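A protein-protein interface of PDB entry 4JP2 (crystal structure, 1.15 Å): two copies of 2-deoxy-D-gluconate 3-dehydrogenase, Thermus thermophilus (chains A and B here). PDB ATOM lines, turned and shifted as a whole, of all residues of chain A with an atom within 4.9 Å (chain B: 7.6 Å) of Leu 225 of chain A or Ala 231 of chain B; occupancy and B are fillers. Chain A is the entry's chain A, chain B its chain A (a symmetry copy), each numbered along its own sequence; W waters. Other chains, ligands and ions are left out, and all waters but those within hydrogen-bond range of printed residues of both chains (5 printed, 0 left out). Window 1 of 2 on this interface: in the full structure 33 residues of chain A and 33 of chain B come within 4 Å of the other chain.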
ATOM      1  N   ARG A 168     -20.207 -28.231 -18.436  1.00  0.00           N
ATOM      2  CA  ARG A 168     -20.123 -27.067 -17.557  1.00  0.00           C
ATOM      3  C   ARG A 168     -21.573 -26.610 -17.397  1.00  0.00           C
ATOM      4  O   ARG A 168     -22.341 -26.616 -18.365  1.00  0.00           O
ATOM      5  CB  ARG A 168     -19.271 -25.955 -18.179  1.00  0.00           C
ATOM      6  CG  ARG A 168     -17.908 -26.418 -18.676  1.00  0.00           C
ATOM      7  CD  ARG A 168     -17.094 -27.095 -17.582  1.00  0.00           C
ATOM      8  NE  ARG A 168     -15.912 -27.764 -18.128  1.00  0.00           N
ATOM      9  CZ  ARG A 168     -15.635 -29.056 -17.978  1.00  0.00           C
ATOM     10  NH1 ARG A 168     -16.454 -29.847 -17.300  1.00  0.00           N
ATOM     11  NH2 ARG A 168     -14.524 -29.559 -18.501  1.00  0.00           N
ATOM     12  N   ASN A 170     -23.924 -23.474 -15.672  1.00  0.00           N
ATOM     13  CA  ASN A 170     -23.930 -22.154 -15.054  1.00  0.00           C
ATOM     14  C   ASN A 170     -25.302 -21.505 -15.126  1.00  0.00           C
ATOM     15  O   ASN A 170     -26.186 -21.965 -15.856  1.00  0.00           O
ATOM     16  CB  ASN A 170     -22.882 -21.262 -15.719  1.00  0.00           C
ATOM     17  CG  ASN A 170     -21.472 -21.768 -15.494  1.00  0.00           C
ATOM     18  OD1 ASN A 170     -20.958 -21.725 -14.378  1.00  0.00           O
ATOM     19  ND2 ASN A 170     -20.846 -22.271 -16.551  1.00  0.00           N
ATOM     20  N   LEU A 217     -20.860 -18.333 -22.084  1.00  0.00           N
ATOM     21  CA  LEU A 217     -21.132 -19.446 -21.185  1.00  0.00           C
ATOM     22  C   LEU A 217     -21.519 -20.727 -21.918  1.00  0.00           C
ATOM     23  O   LEU A 217     -21.594 -21.796 -21.315  1.00  0.00           O
ATOM     24  CB  LEU A 217     -22.206 -19.039 -20.170  1.00  0.00           C
ATOM     25  CG  LEU A 217     -21.759 -17.900 -19.240  1.00  0.00           C
ATOM     26  CD1 LEU A 217     -22.928 -17.433 -18.394  1.00  0.00           C
ATOM     27  CD2 LEU A 217     -20.606 -18.364 -18.357  1.00  0.00           C
ATOM     28  N   ALA A 222     -15.872 -20.805 -21.336  1.00  0.00           N
ATOM     29  CA  ALA A 222     -16.288 -21.327 -20.038  1.00  0.00           C
ATOM     30  C   ALA A 222     -15.706 -22.693 -19.674  1.00  0.00           C
ATOM     31  O   ALA A 222     -16.219 -23.364 -18.781  1.00  0.00           O
ATOM     32  CB  ALA A 222     -17.815 -21.381 -19.974  1.00  0.00           C
ATOM     33  N   GLU A 223     -14.626 -23.096 -20.333  1.00  0.00           N
ATOM     34  CA  GLU A 223     -14.027 -24.393 -20.047  1.00  0.00           C
ATOM     35  C   GLU A 223     -13.753 -24.641 -18.566  1.00  0.00           C
ATOM     36  O   GLU A 223     -13.993 -25.745 -18.079  1.00  0.00           O
ATOM     37  CB  GLU A 223     -12.735 -24.564 -20.850  1.00  0.00           C
ATOM     38  CG  GLU A 223     -11.896 -25.797 -20.499  1.00  0.00           C
ATOM     39  CD  GLU A 223     -12.664 -27.103 -20.562  1.00  0.00           C
ATOM     40  OE1 GLU A 223     -13.588 -27.210 -21.393  1.00  0.00           O
ATOM     41  OE2 GLU A 223     -12.332 -28.032 -19.792  1.00  0.00           O
ATOM     42  N   TYR A 224     -13.257 -23.632 -17.849  1.00  0.00           N
ATOM     43  CA  TYR A 224     -12.959 -23.796 -16.425  1.00  0.00           C
ATOM     44  C   TYR A 224     -13.948 -23.019 -15.551  1.00  0.00           C
ATOM     45  O   TYR A 224     -13.688 -22.773 -14.370  1.00  0.00           O
ATOM     46  CB  TYR A 224     -11.524 -23.331 -16.125  1.00  0.00           C
ATOM     47  CG  TYR A 224     -10.898 -23.986 -14.907  1.00  0.00           C
ATOM     48  CD1 TYR A 224     -10.526 -25.331 -14.930  1.00  0.00           C
ATOM     49  CD2 TYR A 224     -10.696 -23.269 -13.729  1.00  0.00           C
ATOM     50  CE1 TYR A 224      -9.970 -25.947 -13.808  1.00  0.00           C
ATOM     51  CE2 TYR A 224     -10.141 -23.873 -12.602  1.00  0.00           C
ATOM     52  CZ  TYR A 224      -9.782 -25.210 -12.647  1.00  0.00           C
ATOM     53  OH  TYR A 224      -9.248 -25.807 -11.526  1.00  0.00           O
ATOM     54  N   LEU A 225     -15.086 -22.644 -16.133  1.00  0.00           N
ATOM     55  CA  LEU A 225     -16.103 -21.876 -15.422  1.00  0.00           C
ATOM     56  C   LEU A 225     -17.346 -22.745 -15.264  1.00  0.00           C
ATOM     57  O   LEU A 225     -18.054 -23.007 -16.239  1.00  0.00           O
ATOM     58  CB  LEU A 225     -16.432 -20.606 -16.215  1.00  0.00           C
ATOM     59  CG  LEU A 225     -17.046 -19.418 -15.465  1.00  0.00           C
ATOM     60  CD1 LEU A 225     -17.120 -18.221 -16.401  1.00  0.00           C
ATOM     61  CD2 LEU A 225     -18.428 -19.775 -14.934  1.00  0.00           C
ATOM     62  N   THR A 226     -17.609 -23.202 -14.047  1.00  0.00           N
ATOM     63  CA  THR A 226     -18.764 -24.048 -13.829  1.00  0.00           C
ATOM     64  C   THR A 226     -19.283 -23.951 -12.399  1.00  0.00           C
ATOM     65  O   THR A 226     -18.520 -23.697 -11.459  1.00  0.00           O
ATOM     66  CB  THR A 226     -18.427 -25.518 -14.199  1.00  0.00           C
ATOM     67  OG1 THR A 226     -19.639 -26.271 -14.286  1.00  0.00           O
ATOM     68  CG2 THR A 226     -17.491 -26.149 -13.174  1.00  0.00           C
ATOM     69  N   GLY A 227     -20.595 -24.139 -12.259  1.00  0.00           N
ATOM     70  CA  GLY A 227     -21.253 -24.079 -10.965  1.00  0.00           C
ATOM     71  C   GLY A 227     -21.454 -22.670 -10.442  1.00  0.00           C
ATOM     72  O   GLY A 227     -21.629 -22.473  -9.236  1.00  0.00           O
ATOM     73  N   GLN A 228     -21.469 -21.700 -11.350  1.00  0.00           N
ATOM     74  CA  GLN A 228     -21.586 -20.300 -10.980  1.00  0.00           C
ATOM     75  C   GLN A 228     -22.738 -19.533 -11.590  1.00  0.00           C
ATOM     76  O   GLN A 228     -23.257 -19.884 -12.653  1.00  0.00           O
ATOM     77  CB  GLN A 228     -20.306 -19.566 -11.380  1.00  0.00           C
ATOM     78  CG  GLN A 228     -19.085 -19.952 -10.589  1.00  0.00           C
ATOM     79  CD  GLN A 228     -19.206 -19.521  -9.151  1.00  0.00           C
ATOM     80  OE1 GLN A 228     -19.574 -18.382  -8.870  1.00  0.00           O
ATOM     81  NE2 GLN A 228     -18.896 -20.421  -8.230  1.00  0.00           N
ATOM     82  N   VAL A 230     -23.714 -15.818 -13.052  1.00  0.00           N
ATOM     83  CA  VAL A 230     -23.048 -14.663 -13.635  1.00  0.00           C
ATOM     84  C   VAL A 230     -24.157 -13.646 -13.861  1.00  0.00           C
ATOM     85  O   VAL A 230     -25.053 -13.860 -14.683  1.00  0.00           O
ATOM     86  CB  VAL A 230     -22.364 -15.001 -14.981  1.00  0.00           C
ATOM     87  CG1 VAL A 230     -21.763 -13.739 -15.591  1.00  0.00           C
ATOM     88  CG2 VAL A 230     -21.283 -16.050 -14.767  1.00  0.00           C
ATOM     89  N   SER B 129      -9.911 -14.114  -6.074  1.00  0.00           N
ATOM     90  CA  SER B 129      -9.427 -15.442  -5.723  1.00  0.00           C
ATOM     91  C   SER B 129     -10.577 -16.234  -5.121  1.00  0.00           C
ATOM     92  O   SER B 129     -11.655 -15.689  -4.896  1.00  0.00           O
ATOM     93  CB  SER B 129      -8.319 -15.274  -4.674  1.00  0.00           C
ATOM     94  OG  SER B 129      -8.035 -16.467  -3.965  1.00  0.00           O
ATOM     95  N   VAL B 130     -10.372 -17.524  -4.875  1.00  0.00           N
ATOM     96  CA  VAL B 130     -11.429 -18.268  -4.213  1.00  0.00           C
ATOM     97  C   VAL B 130     -11.468 -17.700  -2.793  1.00  0.00           C
ATOM     98  O   VAL B 130     -12.466 -17.852  -2.088  1.00  0.00           O
ATOM     99  CB  VAL B 130     -11.152 -19.793  -4.157  1.00  0.00           C
ATOM    100  CG1 VAL B 130     -11.192 -20.377  -5.556  1.00  0.00           C
ATOM    101  CG2 VAL B 130      -9.817 -20.065  -3.494  1.00  0.00           C
ATOM    102  N   PHE B 133     -14.120 -15.428  -1.347  1.00  0.00           N
ATOM    103  CA  PHE B 133     -15.322 -16.049  -0.791  1.00  0.00           C
ATOM    104  C   PHE B 133     -15.099 -17.038   0.347  1.00  0.00           C
ATOM    105  O   PHE B 133     -16.053 -17.438   1.018  1.00  0.00           O
ATOM    106  CB  PHE B 133     -16.076 -16.747  -1.922  1.00  0.00           C
ATOM    107  CG  PHE B 133     -16.511 -15.812  -3.007  1.00  0.00           C
ATOM    108  CD1 PHE B 133     -17.587 -14.958  -2.805  1.00  0.00           C
ATOM    109  CD2 PHE B 133     -15.814 -15.738  -4.210  1.00  0.00           C
ATOM    110  CE1 PHE B 133     -17.967 -14.040  -3.779  1.00  0.00           C
ATOM    111  CE2 PHE B 133     -16.186 -14.821  -5.194  1.00  0.00           C
ATOM    112  CZ  PHE B 133     -17.264 -13.972  -4.974  1.00  0.00           C
ATOM    113  N   LEU B 171     -14.532  -8.144 -11.004  1.00  0.00           N
ATOM    114  CA  LEU B 171     -13.511  -8.886 -10.289  1.00  0.00           C
ATOM    115  C   LEU B 171     -13.448 -10.328 -10.788  1.00  0.00           C
ATOM    116  O   LEU B 171     -14.351 -11.128 -10.530  1.00  0.00           O
ATOM    117  CB  LEU B 171     -13.832  -8.876  -8.790  1.00  0.00           C
ATOM    118  CG  LEU B 171     -12.844  -9.582  -7.856  1.00  0.00           C
ATOM    119  CD1 LEU B 171     -11.540  -8.802  -7.791  1.00  0.00           C
ATOM    120  CD2 LEU B 171     -13.451  -9.702  -6.465  1.00  0.00           C
ATOM    121  N   LEU B 172     -12.387 -10.654 -11.517  1.00  0.00           N
ATOM    122  CA  LEU B 172     -12.208 -12.014 -12.011  1.00  0.00           C
ATOM    123  C   LEU B 172     -11.575 -12.806 -10.877  1.00  0.00           C
ATOM    124  O   LEU B 172     -10.497 -12.449 -10.399  1.00  0.00           O
ATOM    125  CB  LEU B 172     -11.289 -12.021 -13.230  1.00  0.00           C
ATOM    126  CG  LEU B 172     -10.837 -13.396 -13.726  1.00  0.00           C
ATOM    127  CD1 LEU B 172     -12.037 -14.243 -14.117  1.00  0.00           C
ATOM    128  CD2 LEU B 172      -9.899 -13.215 -14.909  1.00  0.00           C
ATOM    129  N   CYS B 173     -12.245 -13.871 -10.441  1.00  0.00           N
ATOM    130  CA  CYS B 173     -11.748 -14.690  -9.344  1.00  0.00           C
ATOM    131  C   CYS B 173     -11.307 -16.062  -9.823  1.00  0.00           C
ATOM    132  O   CYS B 173     -12.117 -16.987  -9.932  1.00  0.00           O
ATOM    133  CB  CYS B 173     -12.826 -14.845  -8.270  1.00  0.00           C
ATOM    134  SG  CYS B 173     -13.331 -13.285  -7.530  1.00  0.00           S
ATOM    135  N   PRO B 174     -10.010 -16.212 -10.132  1.00  0.00           N
ATOM    136  CA  PRO B 174      -9.501 -17.503 -10.598  1.00  0.00           C
ATOM    137  C   PRO B 174      -9.453 -18.500  -9.453  1.00  0.00           C
ATOM    138  O   PRO B 174      -9.293 -18.120  -8.292  1.00  0.00           O
ATOM    139  CB  PRO B 174      -8.088 -17.177 -11.088  1.00  0.00           C
ATOM    140  CG  PRO B 174      -8.094 -15.684 -11.298  1.00  0.00           C
ATOM    141  CD  PRO B 174      -8.955 -15.187 -10.171  1.00  0.00           C
ATOM    142  N   GLY B 175      -9.593 -19.776  -9.792  1.00  0.00           N
ATOM    143  CA  GLY B 175      -9.502 -20.816  -8.793  1.00  0.00           C
ATOM    144  C   GLY B 175      -8.032 -21.168  -8.653  1.00  0.00           C
ATOM    145  O   GLY B 175      -7.174 -20.283  -8.632  1.00  0.00           O
ATOM    146  N   MET B 201     -13.863 -30.543 -11.408  1.00  0.00           N
ATOM    147  CA  MET B 201     -13.208 -30.875 -12.664  1.00  0.00           C
ATOM    148  C   MET B 201     -11.956 -31.728 -12.472  1.00  0.00           C
ATOM    149  O   MET B 201     -11.421 -32.271 -13.433  1.00  0.00           O
ATOM    150  CB  MET B 201     -12.914 -29.602 -13.457  1.00  0.00           C
ATOM    151  CG  MET B 201     -14.177 -29.072 -14.125  1.00  0.00           C
ATOM    152  SD  MET B 201     -13.957 -27.503 -15.197  1.00  0.00           S
ATOM    153  CE  MET B 201     -12.504 -28.124 -16.310  1.00  0.00           C
ATOM    154  N   GLU B 209      -6.723 -20.640 -19.797  1.00  0.00           N
ATOM    155  CA  GLU B 209      -8.145 -20.892 -19.580  1.00  0.00           C
ATOM    156  C   GLU B 209      -8.775 -19.775 -18.754  1.00  0.00           C
ATOM    157  O   GLU B 209      -9.941 -19.429 -18.950  1.00  0.00           O
ATOM    158  CB  GLU B 209      -8.345 -22.252 -18.901  1.00  0.00           C
ATOM    159  CG  GLU B 209      -7.919 -23.417 -19.793  1.00  0.00           C
ATOM    160  CD  GLU B 209      -7.992 -24.768 -19.109  1.00  0.00           C
ATOM    161  OE1 GLU B 209      -7.591 -24.864 -17.931  1.00  0.00           O
ATOM    162  OE2 GLU B 209      -8.431 -25.745 -19.762  1.00  0.00           O
ATOM    163  N   ILE B 210      -7.998 -19.209 -17.836  1.00  0.00           N
ATOM    164  CA  ILE B 210      -8.472 -18.104 -17.013  1.00  0.00           C
ATOM    165  C   ILE B 210      -8.521 -16.843 -17.883  1.00  0.00           C
ATOM    166  O   ILE B 210      -9.469 -16.054 -17.814  1.00  0.00           O
ATOM    167  CB  ILE B 210      -7.518 -17.851 -15.819  1.00  0.00           C
ATOM    168  CG1 ILE B 210      -7.397 -19.115 -14.959  1.00  0.00           C
ATOM    169  CG2 ILE B 210      -8.007 -16.663 -15.004  1.00  0.00           C
ATOM    170  CD1 ILE B 210      -8.706 -19.611 -14.372  1.00  0.00           C
ATOM    171  N   VAL B 213     -11.651 -15.780 -20.001  1.00  0.00           N
ATOM    172  CA  VAL B 213     -12.710 -15.052 -19.325  1.00  0.00           C
ATOM    173  C   VAL B 213     -12.277 -13.614 -19.050  1.00  0.00           C
ATOM    174  O   VAL B 213     -13.087 -12.691 -19.131  1.00  0.00           O
ATOM    175  CB  VAL B 213     -13.122 -15.771 -18.020  1.00  0.00           C
ATOM    176  CG1 VAL B 213     -14.280 -15.039 -17.365  1.00  0.00           C
ATOM    177  CG2 VAL B 213     -13.517 -17.216 -18.330  1.00  0.00           C
ATOM    178  N   LEU B 217     -14.264  -9.992 -20.044  1.00  0.00           N
ATOM    179  CA  LEU B 217     -14.525  -8.907 -19.110  1.00  0.00           C
ATOM    180  C   LEU B 217     -13.816  -7.610 -19.486  1.00  0.00           C
ATOM    181  O   LEU B 217     -14.083  -6.557 -18.907  1.00  0.00           O
ATOM    182  CB  LEU B 217     -14.158  -9.350 -17.689  1.00  0.00           C
ATOM    183  CG  LEU B 217     -15.024 -10.510 -17.175  1.00  0.00           C
ATOM    184  CD1 LEU B 217     -14.486 -11.009 -15.847  1.00  0.00           C
ATOM    185  CD2 LEU B 217     -16.475 -10.061 -17.034  1.00  0.00           C
ATOM    186  N   GLN B 228     -19.526  -6.925 -10.566  1.00  0.00           N
ATOM    187  CA  GLN B 228     -19.614  -8.336 -10.230  1.00  0.00           C
ATOM    188  C   GLN B 228     -18.308  -9.094 -10.149  1.00  0.00           C
ATOM    189  O   GLN B 228     -17.304  -8.719 -10.759  1.00  0.00           O
ATOM    190  CB  GLN B 228     -20.475  -9.048 -11.273  1.00  0.00           C
ATOM    191  CG  GLN B 228     -21.932  -8.675 -11.249  1.00  0.00           C
ATOM    192  CD  GLN B 228     -22.598  -9.145  -9.982  1.00  0.00           C
ATOM    193  OE1 GLN B 228     -22.428 -10.294  -9.579  1.00  0.00           O
ATOM    194  NE2 GLN B 228     -23.359  -8.269  -9.346  1.00  0.00           N
ATOM    195  N   ALA B 229     -18.349 -10.180  -9.384  1.00  0.00           N
ATOM    196  CA  ALA B 229     -17.230 -11.097  -9.291  1.00  0.00           C
ATOM    197  C   ALA B 229     -17.633 -12.254 -10.210  1.00  0.00           C
ATOM    198  O   ALA B 229     -18.809 -12.639 -10.259  1.00  0.00           O
ATOM    199  CB  ALA B 229     -17.061 -11.602  -7.871  1.00  0.00           C
ATOM    200  N   VAL B 230     -16.672 -12.776 -10.961  1.00  0.00           N
ATOM    201  CA  VAL B 230     -16.913 -13.909 -11.842  1.00  0.00           C
ATOM    202  C   VAL B 230     -15.847 -14.928 -11.466  1.00  0.00           C
ATOM    203  O   VAL B 230     -14.652 -14.699 -11.675  1.00  0.00           O
ATOM    204  CB  VAL B 230     -16.772 -13.530 -13.335  1.00  0.00           C
ATOM    205  CG1 VAL B 230     -16.943 -14.769 -14.206  1.00  0.00           C
ATOM    206  CG2 VAL B 230     -17.807 -12.478 -13.705  1.00  0.00           C
ATOM    207  N   ALA B 231     -16.282 -16.041 -10.884  1.00  0.00           N
ATOM    208  CA  ALA B 231     -15.366 -17.088 -10.451  1.00  0.00           C
ATOM    209  C   ALA B 231     -15.154 -18.135 -11.537  1.00  0.00           C
ATOM    210  O   ALA B 231     -16.113 -18.703 -12.064  1.00  0.00           O
ATOM    211  CB  ALA B 231     -15.893 -17.748  -9.182  1.00  0.00           C
ATOM    212  N   VAL B 232     -13.888 -18.379 -11.861  1.00  0.00           N
ATOM    213  CA  VAL B 232     -13.482 -19.348 -12.883  1.00  0.00           C
ATOM    214  C   VAL B 232     -12.596 -20.303 -12.093  1.00  0.00           C
ATOM    215  O   VAL B 232     -11.369 -20.149 -12.030  1.00  0.00           O
ATOM    216  CB  VAL B 232     -12.698 -18.636 -14.002  1.00  0.00           C
ATOM    217  CG1 VAL B 232     -12.377 -19.607 -15.124  1.00  0.00           C
ATOM    218  CG2 VAL B 232     -13.520 -17.463 -14.528  1.00  0.00           C
ATOM    219  N   ASP B 233     -13.242 -21.306 -11.505  1.00  0.00           N
ATOM    220  CA  ASP B 233     -12.572 -22.204 -10.584  1.00  0.00           C
ATOM    221  C   ASP B 233     -12.788 -23.702 -10.718  1.00  0.00           C
ATOM    222  O   ASP B 233     -12.547 -24.438  -9.760  1.00  0.00           O
ATOM    223  CB  ASP B 233     -12.962 -21.782  -9.166  1.00  0.00           C
ATOM    224  CG  ASP B 233     -14.419 -22.086  -8.847  1.00  0.00           C
ATOM    225  OD1 ASP B 233     -15.157 -22.563  -9.744  1.00  0.00           O
ATOM    226  OD2 ASP B 233     -14.820 -21.852  -7.689  1.00  0.00           O
ATOM    227  N   GLY B 234     -13.245 -24.160 -11.876  1.00  0.00           N
ATOM    228  CA  GLY B 234     -13.439 -25.588 -12.070  1.00  0.00           C
ATOM    229  C   GLY B 234     -14.488 -26.226 -11.180  1.00  0.00           C
ATOM    230  O   GLY B 234     -14.554 -27.457 -11.073  1.00  0.00           O
ATOM    231  N   GLY B 235     -15.310 -25.392 -10.548  1.00  0.00           N
ATOM    232  CA  GLY B 235     -16.361 -25.882  -9.673  1.00  0.00           C
ATOM    233  C   GLY B 235     -16.012 -25.894  -8.196  1.00  0.00           C
ATOM    234  O   GLY B 235     -16.831 -26.298  -7.371  1.00  0.00           O
ATOM    235  N   LEU B 237     -15.773 -23.614  -5.695  1.00  0.00           N
ATOM    236  CA  LEU B 237     -16.681 -22.973  -4.751  1.00  0.00           C
ATOM    237  C   LEU B 237     -18.045 -23.645  -4.674  1.00  0.00           C
ATOM    238  O   LEU B 237     -18.689 -23.635  -3.623  1.00  0.00           O
ATOM    239  CB  LEU B 237     -16.841 -21.487  -5.092  1.00  0.00           C
ATOM    240  CG  LEU B 237     -15.587 -20.629  -4.876  1.00  0.00           C
ATOM    241  CD1 LEU B 237     -15.799 -19.256  -5.491  1.00  0.00           C
ATOM    242  CD2 LEU B 237     -15.277 -20.513  -3.387  1.00  0.00           C
HETATM  243  O   HOH W   1     -16.119 -21.519 -12.085  1.00  0.00           O
HETATM  244  O   HOH W   2      -9.793 -24.372  -9.116  1.00  0.00           O
HETATM  245  O   HOH W   3     -19.213 -16.218 -10.489  1.00  0.00           O
HETATM  246  O   HOH W   4     -12.336 -21.058 -18.882  1.00  0.00           O
HETATM  247  O   HOH W   5     -17.799 -22.985  -8.769  1.00  0.00           O
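Ala 231 of chain B touches two residues of chain A.
Of the printed residues of chain A, Glu 209 of chain B touches Glu 223.
Printed residues of chain A within 4 Å of Asp 233 of chain B: Tyr 224 (3.2 Å) and Thr 226 (3.9 Å).
Of the printed residues of chain A, Leu 237 of chain B touches Gln 228 (3.9 Å).
Of the printed residues of chain B, Glu 223 of chain A touches Met 201 and Glu 209.
Of the printed residues of chain B, Gln 228 of chain A touches Ala 231 (3.5 Å) and Leu 237 (3.9 Å).
The nearest residue of chain B that does not touch Leu 225 of chain A is Val 230 of chain B (4.1 Å).
The nearest printed residue of chain A that does not touch Ala 231 of chain B is Thr 226 of chain A (5.1 Å).
NE of Arg 168 of chain A is in hydrogen-bond range of SD of Met 201 of chain B (3.5 Å).
The backbone carbonyl oxygen (O) of Tyr 224 of chain A sits at hydrogen-bond distance from the backbone NH (N) of Asp 233 of chain B.
The backbone NH (N) of Gly 234 of chain B sits at hydrogen-bond distance from the backbone carbonyl oxygen (O) of Tyr 224 of chain A (2.9 Å).
SD of Met 201 of chain B sits close to O of Glu 223 of chain A.
Water W3 lies within hydrogen-bond range of OE1 of Gln 228 of chain A (2.7 Å) and N of Ala 231 of chain B (3.0 Å).
Water W1 lies within hydrogen-bond range of the side-chain carboxylate of Asp 233 of chain B, the backbone carbonyl oxygen of Ala 231 of chain B and the backbone NH of Thr 226 of chain A.
Water W2 lies within hydrogen-bond range of O of Asp 233 of chain B (2.8 Å) and OH of Tyr 224 of chain A (2.9 Å).
Water W5 lies within hydrogen-bond range of NE2 of Gln 228 of chain A, OD1 of Asp 233 of chain B and O of Thr 226 of chain A.
Water W4 lies within hydrogen-bond range of O of Glu 209 of chain B (2.9 Å), N of Tyr 224 of chain A (2.9 Å) and N of Glu 223 of chain A (3.4 Å).
The guanidinium group (NH2) of Arg 168 of chain A lies within salt-bridge range of the side-chain carboxylate (OE2) of Glu 223 of chain A.
The side-chain amide oxygen (OD1) of Asn 170 of chain A is in hydrogen-bond range of the backbone NH (N) of Gln 228 of chain A, 3.1 Å away.
The backbone NH of Gly 175 of chain B lies within hydrogen-bond range of the backbone carbonyl oxygen of Val 232 of chain B (2.9 Å).
The backbone NH (N) of Met 201 of chain B sits at hydrogen-bond distance from the backbone carbonyl oxygen (O) of Gly 234 of chain B, 3.2 Å away.
The side-chain carboxylate (OD1) of Asp 233 of chain B sits at hydrogen-bond distance from the backbone NH (N) of Gly 235 of chain B, at 2.9 Å.
N of Leu 237 of chain B lies within hydrogen-bond range of OD2 of Asp 233 of chain B (2.8 Å).
Of the 11 printed residues of chain A, 6 touch a printed residue of chain B.
Hydrophobic or aromatic side chains of chain A that line the printed part of chain B: Tyr 224 and Leu 225.
Hydrophobic or aromatic side chains of chain B that line the printed part of chain A: Met 201, Ala 231, Val 232 and Leu 237.
Among the printed residues, 13 pairs touch across the chains.
Among the printed residues, pairs that only touch across the chains: Thr 226 of chain A with Gly 235 of chain B (3.5 Å), Tyr 224 of chain A with Val 232 of chain B (3.5 Å), Glu 223 of chain A with Glu 209 of chain B (3.5 Å), Gln 228 of chain A with Ala 231 of chain B (3.5 Å), Leu 225 of chain A with Ala 231 of chain B (3.6 Å), Thr 226 of chain A with Gly 234 of chain B (3.6 Å), Tyr 224 of chain A with Met 201 of chain B (3.7 Å), Gln 228 of chain A with Leu 237 of chain B (3.9 Å) and Thr 226 of chain A with Asp 233 of chain B (3.9 Å).
3 positions are printed for both chains.
Of the 13 pairs that touch across the chains among the printed residues, none has its exchanged pair printed and touching as well.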
